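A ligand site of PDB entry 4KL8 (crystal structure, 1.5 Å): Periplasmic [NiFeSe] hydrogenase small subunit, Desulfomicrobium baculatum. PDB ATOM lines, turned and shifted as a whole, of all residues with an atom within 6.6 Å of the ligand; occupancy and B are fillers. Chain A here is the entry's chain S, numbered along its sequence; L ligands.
A ring nitrogen (ND1) of His 208 is bound to an iron atom (FE3) of the ligand, 2.1 Å away. SG of Cys 231 is bound to FE1 of the ligand (2.3 Å). SG of Cys 211 binds FE2 of the ligand. An iron atom (FE4) of the ligand is bound by the side-chain sulfur (SG) of Cys 237 (2.3 Å). S3 of the ligand lies close to N of Lys 232, at 3.3 Å. The backbone NH of Leu 214 lies close to a sulfur (S4) of the ligand, 3.8 Å away.
The backbone NH (N) of His 208 is in hydrogen-bond range of the backbone carbonyl oxygen (O) of Gly 239. N of Ala 233 sits close to SG of Cys 231 (3.3 Å). SG of Cys 211 sits close to N of Tyr 213 (3.4 Å). N of Cys 237 is in hydrogen-bond range of O of Lys 232, at 3.4 Å. The backbone NH (N) of Gly 239 lies close to the side-chain sulfur (SG) of Cys 237 (3.5 Å). The side-chain sulfur (SG) of Cys 237 lies close to the backbone NH (N) of Cys 264 (3.8 Å). NZ of Lys 232 lies within hydrogen-bond range of O of Val 259 (2.7 Å). The side-chain amino group of Lys 232 is in hydrogen-bond range of the backbone carbonyl oxygen of Ala 262, 2.9 Å away.
The backbone carbonyl oxygen (O) of Tyr 213 lies close to a sulfur (S4) of the ligand (3.8 Å). CG2 of Ile 207 touches S1 of the ligand, at 3.97 Å. Tyr 217 touches the ligand (CB to S4, 3.9 Å). CB of Ala 233 touches S2 of the ligand (3.7 Å). Gly 239 touches the ligand. Pro 240 touches the ligand. CG1 of Val 259 touches S3 of the ligand, at 3.5 Å. Hydrophobic or aromatic side chains that line the ligand: Ile 207, His 208, Tyr 213, Tyr 217, Ala 233, Pro 240 and Val 259. Within 4 Å of the ligand: Ile 207, His 208, Cys 211, Tyr 213, Leu 214, Tyr 217, Cys 231, Lys 232, Ala 233, Cys 237, Gly 239, Pro 240 and Val 259. The nearest printed residue that does not touch the ligand is Lys 238 (5.4 Å).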
ATOM      1  N   ILE A 207      -8.340 -17.523 -10.559  1.00  0.00           N
ATOM      2  CA  ILE A 207      -7.310 -18.583 -10.580  1.00  0.00           C
ATOM      3  C   ILE A 207      -7.256 -19.272 -11.947  1.00  0.00           C
ATOM      4  O   ILE A 207      -6.188 -19.333 -12.566  1.00  0.00           O
ATOM      5  CB  ILE A 207      -7.571 -19.602  -9.462  1.00  0.00           C
ATOM      6  CG1 ILE A 207      -7.459 -18.910  -8.090  1.00  0.00           C
ATOM      7  CG2 ILE A 207      -6.697 -20.874  -9.659  1.00  0.00           C
ATOM      8  CD1 ILE A 207      -6.218 -19.189  -7.286  1.00  0.00           C
ATOM      9  N   HIS A 208      -8.397 -19.767 -12.410  1.00  0.00           N
ATOM     10  CA  HIS A 208      -8.494 -20.505 -13.669  1.00  0.00           C
ATOM     11  C   HIS A 208      -7.984 -19.683 -14.870  1.00  0.00           C
ATOM     12  O   HIS A 208      -7.157 -20.169 -15.663  1.00  0.00           O
ATOM     13  CB  HIS A 208      -9.946 -20.980 -13.822  1.00  0.00           C
ATOM     14  CG  HIS A 208     -10.246 -21.705 -15.091  1.00  0.00           C
ATOM     15  ND1 HIS A 208      -9.890 -23.018 -15.314  1.00  0.00           N
ATOM     16  CD2 HIS A 208     -10.922 -21.299 -16.188  1.00  0.00           C
ATOM     17  CE1 HIS A 208     -10.321 -23.387 -16.511  1.00  0.00           C
ATOM     18  NE2 HIS A 208     -10.946 -22.355 -17.067  1.00  0.00           N
ATOM     19  N   GLU A 209      -8.410 -18.424 -14.979  1.00  0.00           N
ATOM     20  CA  GLU A 209      -7.991 -17.590 -16.114  1.00  0.00           C
ATOM     21  C   GLU A 209      -6.485 -17.440 -16.147  1.00  0.00           C
ATOM     22  O   GLU A 209      -5.889 -17.249 -17.212  1.00  0.00           O
ATOM     23  CB  GLU A 209      -8.684 -16.232 -16.085  1.00  0.00           C
ATOM     24  CG  GLU A 209     -10.191 -16.303 -16.317  1.00  0.00           C
ATOM     25  CD  GLU A 209     -10.883 -14.953 -16.171  1.00  0.00           C
ATOM     26  OE1 GLU A 209     -10.208 -13.894 -16.179  1.00  0.00           O
ATOM     27  OE2 GLU A 209     -12.118 -14.946 -16.041  1.00  0.00           O
ATOM     28  N   CYS A 211      -4.285 -19.753 -14.827  1.00  0.00           N
ATOM     29  CA  CYS A 211      -3.694 -21.033 -14.451  1.00  0.00           C
ATOM     30  C   CYS A 211      -2.762 -21.569 -15.541  1.00  0.00           C
ATOM     31  O   CYS A 211      -3.114 -21.538 -16.718  1.00  0.00           O
ATOM     32  CB  CYS A 211      -4.784 -22.047 -14.147  1.00  0.00           C
ATOM     33  SG  CYS A 211      -4.165 -23.642 -13.618  1.00  0.00           S
ATOM     34  N   PRO A 212      -1.597 -22.102 -15.148  1.00  0.00           N
ATOM     35  CA  PRO A 212      -0.695 -22.694 -16.154  1.00  0.00           C
ATOM     36  C   PRO A 212      -1.263 -23.969 -16.838  1.00  0.00           C
ATOM     37  O   PRO A 212      -0.713 -24.409 -17.852  1.00  0.00           O
ATOM     38  CB  PRO A 212       0.565 -23.029 -15.361  1.00  0.00           C
ATOM     39  CG  PRO A 212       0.142 -23.124 -13.927  1.00  0.00           C
ATOM     40  CD  PRO A 212      -1.024 -22.169 -13.780  1.00  0.00           C
ATOM     41  N   TYR A 213      -2.334 -24.544 -16.287  1.00  0.00           N
ATOM     42  CA  TYR A 213      -2.966 -25.720 -16.889  1.00  0.00           C
ATOM     43  C   TYR A 213      -4.055 -25.342 -17.888  1.00  0.00           C
ATOM     44  O   TYR A 213      -4.727 -26.230 -18.412  1.00  0.00           O
ATOM     45  CB  TYR A 213      -3.572 -26.638 -15.819  1.00  0.00           C
ATOM     46  CG  TYR A 213      -2.589 -27.355 -14.939  1.00  0.00           C
ATOM     47  CD1 TYR A 213      -2.088 -26.742 -13.779  1.00  0.00           C
ATOM     48  CD2 TYR A 213      -2.219 -28.688 -15.191  1.00  0.00           C
ATOM     49  CE1 TYR A 213      -1.166 -27.399 -12.958  1.00  0.00           C
ATOM     50  CE2 TYR A 213      -1.318 -29.370 -14.342  1.00  0.00           C
ATOM     51  CZ  TYR A 213      -0.796 -28.713 -13.233  1.00  0.00           C
ATOM     52  OH  TYR A 213       0.087 -29.334 -12.386  1.00  0.00           O
ATOM     53  N   LEU A 214      -4.254 -24.041 -18.132  1.00  0.00           N
ATOM     54  CA  LEU A 214      -5.382 -23.616 -18.944  1.00  0.00           C
ATOM     55  C   LEU A 214      -5.301 -24.172 -20.368  1.00  0.00           C
ATOM     56  O   LEU A 214      -6.322 -24.510 -20.962  1.00  0.00           O
ATOM     57  CB  LEU A 214      -5.554 -22.081 -18.938  1.00  0.00           C
ATOM     58  CG  LEU A 214      -6.842 -21.537 -19.569  1.00  0.00           C
ATOM     59  CD1 LEU A 214      -8.099 -21.985 -18.812  1.00  0.00           C
ATOM     60  CD2 LEU A 214      -6.783 -20.017 -19.590  1.00  0.00           C
ATOM     61  N   ASP A 215      -4.078 -24.298 -20.917  1.00  0.00           N
ATOM     62  CA  ASP A 215      -3.923 -24.890 -22.251  1.00  0.00           C
ATOM     63  C   ASP A 215      -4.430 -26.343 -22.273  1.00  0.00           C
ATOM     64  O   ASP A 215      -5.083 -26.781 -23.224  1.00  0.00           O
ATOM     65  CB  ASP A 215      -2.453 -24.778 -22.737  1.00  0.00           C
ATOM     66  CG  ASP A 215      -1.434 -25.519 -21.826  1.00  0.00           C
ATOM     67  OD1 ASP A 215      -1.684 -25.769 -20.616  1.00  0.00           O
ATOM     68  OD2 ASP A 215      -0.345 -25.843 -22.356  1.00  0.00           O
ATOM     69  N   LYS A 216      -4.168 -27.063 -21.188  1.00  0.00           N
ATOM     70  CA  LYS A 216      -4.609 -28.448 -21.084  1.00  0.00           C
ATOM     71  C   LYS A 216      -6.132 -28.526 -20.958  1.00  0.00           C
ATOM     72  O   LYS A 216      -6.777 -29.332 -21.640  1.00  0.00           O
ATOM     73  CB  LYS A 216      -3.909 -29.157 -19.935  1.00  0.00           C
ATOM     74  CG  LYS A 216      -2.384 -29.282 -20.132  1.00  0.00           C
ATOM     75  CD  LYS A 216      -1.694 -29.896 -18.921  1.00  0.00           C
ATOM     76  CE  LYS A 216      -0.182 -29.648 -18.919  1.00  0.00           C
ATOM     77  NZ  LYS A 216       0.401 -29.606 -20.286  1.00  0.00           N
ATOM     78  N   TYR A 217      -6.696 -27.690 -20.099  1.00  0.00           N
ATOM     79  CA  TYR A 217      -8.139 -27.549 -19.995  1.00  0.00           C
ATOM     80  C   TYR A 217      -8.775 -27.318 -21.377  1.00  0.00           C
ATOM     81  O   TYR A 217      -9.771 -27.963 -21.747  1.00  0.00           O
ATOM     82  CB  TYR A 217      -8.470 -26.384 -19.034  1.00  0.00           C
ATOM     83  CG  TYR A 217      -9.939 -26.071 -18.909  1.00  0.00           C
ATOM     84  CD1 TYR A 217     -10.549 -25.174 -19.790  1.00  0.00           C
ATOM     85  CD2 TYR A 217     -10.728 -26.654 -17.898  1.00  0.00           C
ATOM     86  CE1 TYR A 217     -11.915 -24.880 -19.702  1.00  0.00           C
ATOM     87  CE2 TYR A 217     -12.099 -26.346 -17.791  1.00  0.00           C
ATOM     88  CZ  TYR A 217     -12.669 -25.454 -18.693  1.00  0.00           C
ATOM     89  OH  TYR A 217     -14.008 -25.160 -18.589  1.00  0.00           O
ATOM     90  N   PHE A 222      -7.521 -33.821 -19.198  1.00  0.00           N
ATOM     91  CA  PHE A 222      -7.812 -33.840 -17.774  1.00  0.00           C
ATOM     92  C   PHE A 222      -7.130 -34.993 -17.046  1.00  0.00           C
ATOM     93  O   PHE A 222      -7.209 -36.147 -17.482  1.00  0.00           O
ATOM     94  CB  PHE A 222      -9.319 -33.891 -17.525  1.00  0.00           C
ATOM     95  CG  PHE A 222     -10.064 -32.745 -18.146  1.00  0.00           C
ATOM     96  CD1 PHE A 222      -9.970 -31.456 -17.623  1.00  0.00           C
ATOM     97  CD2 PHE A 222     -10.850 -32.955 -19.280  1.00  0.00           C
ATOM     98  CE1 PHE A 222     -10.654 -30.396 -18.203  1.00  0.00           C
ATOM     99  CE2 PHE A 222     -11.540 -31.908 -19.858  1.00  0.00           C
ATOM    100  CZ  PHE A 222     -11.438 -30.615 -19.341  1.00  0.00           C
ATOM    101  N   GLY A 230      -2.373 -33.464 -16.795  1.00  0.00           N
ATOM    102  CA  GLY A 230      -3.589 -32.800 -17.257  1.00  0.00           C
ATOM    103  C   GLY A 230      -4.143 -31.774 -16.285  1.00  0.00           C
ATOM    104  O   GLY A 230      -3.717 -31.670 -15.137  1.00  0.00           O
ATOM    105  N   CYS A 231      -5.124 -30.999 -16.760  1.00  0.00           N
ATOM    106  CA  CYS A 231      -5.868 -30.083 -15.907  1.00  0.00           C
ATOM    107  C   CYS A 231      -6.538 -30.858 -14.761  1.00  0.00           C
ATOM    108  O   CYS A 231      -6.918 -32.033 -14.917  1.00  0.00           O
ATOM    109  CB  CYS A 231      -6.879 -29.330 -16.783  1.00  0.00           C
ATOM    110  SG  CYS A 231      -8.259 -28.592 -15.916  1.00  0.00           S
ATOM    111  N   LYS A 232      -6.702 -30.206 -13.609  1.00  0.00           N
ATOM    112  CA  LYS A 232      -7.254 -30.837 -12.396  1.00  0.00           C
ATOM    113  C   LYS A 232      -8.781 -30.733 -12.267  1.00  0.00           C
ATOM    114  O   LYS A 232      -9.331 -31.115 -11.244  1.00  0.00           O
ATOM    115  CB  LYS A 232      -6.611 -30.188 -11.154  1.00  0.00           C
ATOM    116  CG  LYS A 232      -5.088 -30.099 -11.185  1.00  0.00           C
ATOM    117  CD  LYS A 232      -4.431 -31.508 -11.310  1.00  0.00           C
ATOM    118  CE  LYS A 232      -2.925 -31.437 -11.078  1.00  0.00           C
ATOM    119  NZ  LYS A 232      -2.601 -31.247  -9.644  1.00  0.00           N
ATOM    120  N   ALA A 233      -9.476 -30.226 -13.291  1.00  0.00           N
ATOM    121  CA  ALA A 233     -10.920 -29.953 -13.194  1.00  0.00           C
ATOM    122  C   ALA A 233     -11.734 -31.182 -12.774  1.00  0.00           C
ATOM    123  O   ALA A 233     -12.643 -31.068 -11.953  1.00  0.00           O
ATOM    124  CB  ALA A 233     -11.467 -29.412 -14.512  1.00  0.00           C
ATOM    125  N   GLU A 234     -11.429 -32.352 -13.356  1.00  0.00           N
ATOM    126  CA  GLU A 234     -12.214 -33.551 -13.036  1.00  0.00           C
ATOM    127  C   GLU A 234     -11.940 -34.087 -11.629  1.00  0.00           C
ATOM    128  O   GLU A 234     -12.716 -34.886 -11.084  1.00  0.00           O
ATOM    129  CB  GLU A 234     -12.013 -34.650 -14.088  1.00  0.00           C
ATOM    130  CG  GLU A 234     -12.511 -34.304 -15.465  1.00  0.00           C
ATOM    131  CD  GLU A 234     -12.278 -35.413 -16.465  1.00  0.00           C
ATOM    132  OE1 GLU A 234     -12.676 -35.258 -17.625  1.00  0.00           O
ATOM    133  OE2 GLU A 234     -11.664 -36.443 -16.113  1.00  0.00           O
ATOM    134  N   CYS A 237     -11.135 -29.404  -8.940  1.00  0.00           N
ATOM    135  CA  CYS A 237     -10.556 -28.053  -8.889  1.00  0.00           C
ATOM    136  C   CYS A 237     -11.607 -26.953  -8.938  1.00  0.00           C
ATOM    137  O   CYS A 237     -12.447 -26.920  -9.870  1.00  0.00           O
ATOM    138  CB  CYS A 237      -9.551 -27.866 -10.025  1.00  0.00           C
ATOM    139  SG  CYS A 237      -8.584 -26.339  -9.856  1.00  0.00           S
ATOM    140  N   LYS A 238     -11.563 -26.052  -7.940  1.00  0.00           N
ATOM    141  CA  LYS A 238     -12.471 -24.888  -7.890  1.00  0.00           C
ATOM    142  C   LYS A 238     -11.828 -23.596  -8.418  1.00  0.00           C
ATOM    143  O   LYS A 238     -12.378 -22.507  -8.235  1.00  0.00           O
ATOM    144  CB  LYS A 238     -13.072 -24.689  -6.484  1.00  0.00           C
ATOM    145  CG  LYS A 238     -13.734 -25.944  -5.920  1.00  0.00           C
ATOM    146  CD  LYS A 238     -14.808 -26.496  -6.872  1.00  0.00           C
ATOM    147  CE  LYS A 238     -15.661 -27.620  -6.245  1.00  0.00           C
ATOM    148  NZ  LYS A 238     -14.836 -28.713  -5.697  1.00  0.00           N
ATOM    149  N   GLY A 239     -10.703 -23.717  -9.107  1.00  0.00           N
ATOM    150  CA  GLY A 239     -10.071 -22.560  -9.753  1.00  0.00           C
ATOM    151  C   GLY A 239     -11.012 -21.710 -10.582  1.00  0.00           C
ATOM    152  O   GLY A 239     -10.909 -20.478 -10.553  1.00  0.00           O
ATOM    153  N   PRO A 240     -11.946 -22.342 -11.335  1.00  0.00           N
ATOM    154  CA  PRO A 240     -12.881 -21.584 -12.144  1.00  0.00           C
ATOM    155  C   PRO A 240     -13.741 -20.553 -11.385  1.00  0.00           C
ATOM    156  O   PRO A 240     -14.082 -19.517 -11.959  1.00  0.00           O
ATOM    157  CB  PRO A 240     -13.748 -22.684 -12.772  1.00  0.00           C
ATOM    158  CG  PRO A 240     -12.748 -23.770 -13.022  1.00  0.00           C
ATOM    159  CD  PRO A 240     -12.006 -23.789 -11.686  1.00  0.00           C
ATOM    160  N   TRP A 257       2.078 -24.967  -4.972  1.00  0.00           N
ATOM    161  CA  TRP A 257       0.729 -24.399  -4.726  1.00  0.00           C
ATOM    162  C   TRP A 257      -0.339 -25.454  -4.923  1.00  0.00           C
ATOM    163  O   TRP A 257      -0.051 -26.542  -5.439  1.00  0.00           O
ATOM    164  CB  TRP A 257       0.434 -23.151  -5.544  1.00  0.00           C
ATOM    165  CG  TRP A 257       0.273 -23.363  -7.028  1.00  0.00           C
ATOM    166  CD1 TRP A 257       1.170 -23.949  -7.897  1.00  0.00           C
ATOM    167  CD2 TRP A 257      -0.825 -22.911  -7.836  1.00  0.00           C
ATOM    168  NE1 TRP A 257       0.689 -23.888  -9.185  1.00  0.00           N
ATOM    169  CE2 TRP A 257      -0.549 -23.281  -9.174  1.00  0.00           C
ATOM    170  CE3 TRP A 257      -2.028 -22.248  -7.554  1.00  0.00           C
ATOM    171  CZ2 TRP A 257      -1.417 -22.992 -10.242  1.00  0.00           C
ATOM    172  CZ3 TRP A 257      -2.907 -21.959  -8.601  1.00  0.00           C
ATOM    173  CH2 TRP A 257      -2.602 -22.333  -9.938  1.00  0.00           C
ATOM    174  N   VAL A 259      -2.963 -26.068  -6.797  1.00  0.00           N
ATOM    175  CA  VAL A 259      -3.323 -26.589  -8.103  1.00  0.00           C
ATOM    176  C   VAL A 259      -2.247 -27.507  -8.672  1.00  0.00           C
ATOM    177  O   VAL A 259      -2.579 -28.576  -9.170  1.00  0.00           O
ATOM    178  CB  VAL A 259      -3.717 -25.450  -9.079  1.00  0.00           C
ATOM    179  CG1 VAL A 259      -3.929 -26.000 -10.491  1.00  0.00           C
ATOM    180  CG2 VAL A 259      -4.998 -24.763  -8.569  1.00  0.00           C
ATOM    181  N   ALA A 262      -2.374 -30.593  -6.270  1.00  0.00           N
ATOM    182  CA  ALA A 262      -3.649 -31.297  -6.079  1.00  0.00           C
ATOM    183  C   ALA A 262      -4.777 -30.532  -6.748  1.00  0.00           C
ATOM    184  O   ALA A 262      -4.872 -30.570  -7.970  1.00  0.00           O
ATOM    185  CB  ALA A 262      -3.932 -31.549  -4.564  1.00  0.00           C
ATOM    186  N   VAL A 263      -5.618 -29.871  -5.969  1.00  0.00           N
ATOM    187  CA  VAL A 263      -6.722 -29.049  -6.504  1.00  0.00           C
ATOM    188  C   VAL A 263      -6.834 -27.759  -5.672  1.00  0.00           C
ATOM    189  O   VAL A 263      -6.421 -27.717  -4.509  1.00  0.00           O
ATOM    190  CB  VAL A 263      -8.105 -29.783  -6.451  1.00  0.00           C
ATOM    191  CG1 VAL A 263      -8.182 -30.963  -7.475  1.00  0.00           C
ATOM    192  CG2 VAL A 263      -8.431 -30.253  -5.023  1.00  0.00           C
ATOM    193  N   CYS A 264      -7.389 -26.714  -6.286  1.00  0.00           N
ATOM    194  CA  CYS A 264      -7.854 -25.537  -5.540  1.00  0.00           C
ATOM    195  C   CYS A 264      -9.189 -25.913  -4.890  1.00  0.00           C
ATOM    196  O   CYS A 264     -10.047 -26.522  -5.532  1.00  0.00           O
ATOM    197  CB  CYS A 264      -8.011 -24.325  -6.481  1.00  0.00           C
ATOM    198  SG  CYS A 264      -8.725 -22.842  -5.689  1.00  0.00           S
HETATM  199 FE1  LIG L   1      -7.709 -26.763 -14.682  1.00  0.00          FE
HETATM  200 FE2  LIG L   1      -6.144 -24.801 -13.688  1.00  0.00          FE
HETATM  201 FE3  LIG L   1      -8.695 -24.336 -14.243  1.00  0.00          FE
HETATM  202 FE4  LIG L   1      -8.054 -25.916 -12.061  1.00  0.00          FE
HETATM  203  S1  LIG L   1      -7.652 -23.668 -12.320  1.00  0.00           S
HETATM  204  S2  LIG L   1      -9.683 -26.309 -13.587  1.00  0.00           S
HETATM  205  S3  LIG L   1      -6.214 -26.965 -12.985  1.00  0.00           S
HETATM  206  S4  LIG L   1      -7.070 -24.873 -15.767  1.00  0.00           S
